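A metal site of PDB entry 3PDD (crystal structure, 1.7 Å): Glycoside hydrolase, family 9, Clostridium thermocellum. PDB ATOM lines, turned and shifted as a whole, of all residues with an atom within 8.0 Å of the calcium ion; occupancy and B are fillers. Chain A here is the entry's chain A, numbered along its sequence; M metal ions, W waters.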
ATOM      1  N   PHE A 129     -27.663   3.112 -28.815  1.00  0.00           N
ATOM      2  CA  PHE A 129     -26.535   2.631 -29.576  1.00  0.00           C
ATOM      3  C   PHE A 129     -26.744   1.213 -29.884  1.00  0.00           C
ATOM      4  O   PHE A 129     -27.066   0.451 -28.999  1.00  0.00           O
ATOM      5  CB  PHE A 129     -25.275   2.804 -28.727  1.00  0.00           C
ATOM      6  CG  PHE A 129     -24.932   4.261 -28.452  1.00  0.00           C
ATOM      7  CD1 PHE A 129     -23.969   4.909 -29.209  1.00  0.00           C
ATOM      8  CD2 PHE A 129     -25.556   4.929 -27.426  1.00  0.00           C
ATOM      9  CE1 PHE A 129     -23.665   6.234 -28.977  1.00  0.00           C
ATOM     10  CE2 PHE A 129     -25.273   6.256 -27.207  1.00  0.00           C
ATOM     11  CZ  PHE A 129     -24.353   6.908 -27.987  1.00  0.00           C
ATOM     12  N   SER A 138     -27.720   3.058 -23.963  1.00  0.00           N
ATOM     13  CA  SER A 138     -28.423   4.293 -24.199  1.00  0.00           C
ATOM     14  C   SER A 138     -27.610   5.365 -23.434  1.00  0.00           C
ATOM     15  O   SER A 138     -26.827   5.036 -22.480  1.00  0.00           O
ATOM     16  CB  SER A 138     -29.861   4.250 -23.687  1.00  0.00           C
ATOM     17  OG  SER A 138     -30.585   3.130 -24.179  1.00  0.00           O
ATOM     18  N   ASP A 139     -27.726   6.604 -23.908  1.00  0.00           N
ATOM     19  CA  ASP A 139     -27.178   7.787 -23.243  1.00  0.00           C
ATOM     20  C   ASP A 139     -28.277   8.861 -23.250  1.00  0.00           C
ATOM     21  O   ASP A 139     -28.771   9.241 -24.304  1.00  0.00           O
ATOM     22  CB  ASP A 139     -25.963   8.281 -23.978  1.00  0.00           C
ATOM     23  CG  ASP A 139     -25.165   9.311 -23.202  1.00  0.00           C
ATOM     24  OD1 ASP A 139     -25.664   9.877 -22.170  1.00  0.00           O
ATOM     25  OD2 ASP A 139     -23.993   9.554 -23.600  1.00  0.00           O
ATOM     26  N   ARG A 140     -28.621   9.337 -22.047  1.00  0.00           N
ATOM     27  CA  ARG A 140     -29.708  10.285 -21.841  1.00  0.00           C
ATOM     28  C   ARG A 140     -29.232  11.727 -21.810  1.00  0.00           C
ATOM     29  O   ARG A 140     -30.031  12.668 -21.685  1.00  0.00           O
ATOM     30  CB  ARG A 140     -30.352   9.993 -20.487  1.00  0.00           C
ATOM     31  CG  ARG A 140     -30.772   8.558 -20.307  1.00  0.00           C
ATOM     32  CD  ARG A 140     -31.999   8.515 -19.426  1.00  0.00           C
ATOM     33  NE  ARG A 140     -33.184   8.985 -20.141  1.00  0.00           N
ATOM     34  CZ  ARG A 140     -34.063   8.174 -20.715  1.00  0.00           C
ATOM     35  NH1 ARG A 140     -35.114   8.665 -21.366  1.00  0.00           N
ATOM     36  NH2 ARG A 140     -33.869   6.860 -20.645  1.00  0.00           N
ATOM     37  N   GLU A 141     -27.906  11.923 -21.869  1.00  0.00           N
ATOM     38  CA  GLU A 141     -27.328  13.280 -21.704  1.00  0.00           C
ATOM     39  C   GLU A 141     -26.211  13.520 -22.654  1.00  0.00           C
ATOM     40  O   GLU A 141     -25.223  12.774 -22.660  1.00  0.00           O
ATOM     41  CB  GLU A 141     -26.761  13.545 -20.292  1.00  0.00           C
ATOM     42  CG  GLU A 141     -27.660  13.147 -19.126  1.00  0.00           C
ATOM     43  CD  GLU A 141     -28.960  13.909 -19.078  1.00  0.00           C
ATOM     44  OE1 GLU A 141     -28.987  15.087 -19.544  1.00  0.00           O
ATOM     45  OE2 GLU A 141     -29.936  13.314 -18.542  1.00  0.00           O
ATOM     46  N   ALA A 142     -26.341  14.598 -23.427  1.00  0.00           N
ATOM     47  CA  ALA A 142     -25.286  15.084 -24.281  1.00  0.00           C
ATOM     48  C   ALA A 142     -24.036  15.423 -23.440  1.00  0.00           C
ATOM     49  O   ALA A 142     -24.170  16.017 -22.337  1.00  0.00           O
ATOM     50  CB  ALA A 142     -25.780  16.322 -25.053  1.00  0.00           C
ATOM     51  N   PRO A 143     -22.852  15.066 -23.939  1.00  0.00           N
ATOM     52  CA  PRO A 143     -22.613  14.409 -25.214  1.00  0.00           C
ATOM     53  C   PRO A 143     -23.003  12.943 -25.210  1.00  0.00           C
ATOM     54  O   PRO A 143     -22.794  12.235 -24.170  1.00  0.00           O
ATOM     55  CB  PRO A 143     -21.102  14.557 -25.420  1.00  0.00           C
ATOM     56  CG  PRO A 143     -20.530  14.746 -24.069  1.00  0.00           C
ATOM     57  CD  PRO A 143     -21.613  15.521 -23.307  1.00  0.00           C
ATOM     58  N   TYR A 144     -23.465  12.469 -26.378  1.00  0.00           N
ATOM     59  CA  TYR A 144     -23.951  11.110 -26.531  1.00  0.00           C
ATOM     60  C   TYR A 144     -22.775  10.179 -26.861  1.00  0.00           C
ATOM     61  O   TYR A 144     -22.109  10.335 -27.895  1.00  0.00           O
ATOM     62  CB  TYR A 144     -25.057  11.047 -27.566  1.00  0.00           C
ATOM     63  CG  TYR A 144     -26.212  11.914 -27.191  1.00  0.00           C
ATOM     64  CD1 TYR A 144     -26.978  11.644 -26.061  1.00  0.00           C
ATOM     65  CD2 TYR A 144     -26.510  13.068 -27.922  1.00  0.00           C
ATOM     66  CE1 TYR A 144     -28.056  12.475 -25.668  1.00  0.00           C
ATOM     67  CE2 TYR A 144     -27.539  13.910 -27.525  1.00  0.00           C
ATOM     68  CZ  TYR A 144     -28.337  13.612 -26.459  1.00  0.00           C
ATOM     69  OH  TYR A 144     -29.358  14.477 -26.063  1.00  0.00           O
ATOM     70  N   GLU A 145     -22.544   9.196 -25.959  1.00  0.00           N
ATOM     71  CA  GLU A 145     -21.348   8.357 -26.033  1.00  0.00           C
ATOM     72  C   GLU A 145     -21.683   6.966 -25.493  1.00  0.00           C
ATOM     73  O   GLU A 145     -22.493   6.816 -24.596  1.00  0.00           O
ATOM     74  CB  GLU A 145     -20.223   9.010 -25.142  1.00  0.00           C
ATOM     75  CG  GLU A 145     -19.647  10.345 -25.667  1.00  0.00           C
ATOM     76  CD  GLU A 145     -18.734  11.002 -24.639  1.00  0.00           C
ATOM     77  OE1 GLU A 145     -19.015  10.805 -23.409  1.00  0.00           O
ATOM     78  OE2 GLU A 145     -17.827  11.771 -25.040  1.00  0.00           O
ATOM     79  N   TYR A 146     -21.015   5.933 -26.010  1.00  0.00           N
ATOM     80  CA  TYR A 146     -21.106   4.591 -25.365  1.00  0.00           C
ATOM     81  C   TYR A 146     -19.851   3.841 -25.701  1.00  0.00           C
ATOM     82  O   TYR A 146     -19.329   3.974 -26.800  1.00  0.00           O
ATOM     83  CB  TYR A 146     -22.352   3.810 -25.812  1.00  0.00           C
ATOM     84  CG  TYR A 146     -22.611   2.638 -24.881  1.00  0.00           C
ATOM     85  CD1 TYR A 146     -23.266   2.819 -23.709  1.00  0.00           C
ATOM     86  CD2 TYR A 146     -22.109   1.364 -25.176  1.00  0.00           C
ATOM     87  CE1 TYR A 146     -23.464   1.770 -22.843  1.00  0.00           C
ATOM     88  CE2 TYR A 146     -22.319   0.318 -24.323  1.00  0.00           C
ATOM     89  CZ  TYR A 146     -22.966   0.527 -23.144  1.00  0.00           C
ATOM     90  OH  TYR A 146     -23.175  -0.501 -22.256  1.00  0.00           O
HETATM   91 CA    CA M   1     -23.505  11.410 -22.181  1.00  0.00          CA
HETATM   92  O   HOH W   1     -22.872  13.090 -20.728  1.00  0.00           O
HETATM   93  O   HOH W   2     -24.010  10.576 -20.033  1.00  0.00           O
HETATM   94  O   HOH W   3     -21.373  10.548 -21.829  1.00  0.00           O
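The side-chain carboxylate (OD2) of Asp 139 lies close to the backbone NH (N) of Glu 145.
Three residues have an atom within 4 Å of the calcium ion: Asp 139, Glu 141 and Pro 143.
Along chain A the residues within 4 Å of the calcium ion span positions 139 to 143.
The nearest printed residue that does not touch the calcium ion is Ala 142 (4.2 Å).
The calcium ion is bound by O of Glu 141 (2.2 Å), O of Pro 143 (2.3 Å), water W1 (2.3 Å), water W3 (2.3 Å), water W2 (2.4 Å), OD2 of Asp 139 (2.4 Å) and OD1 of Asp 139 (2.6 Å).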
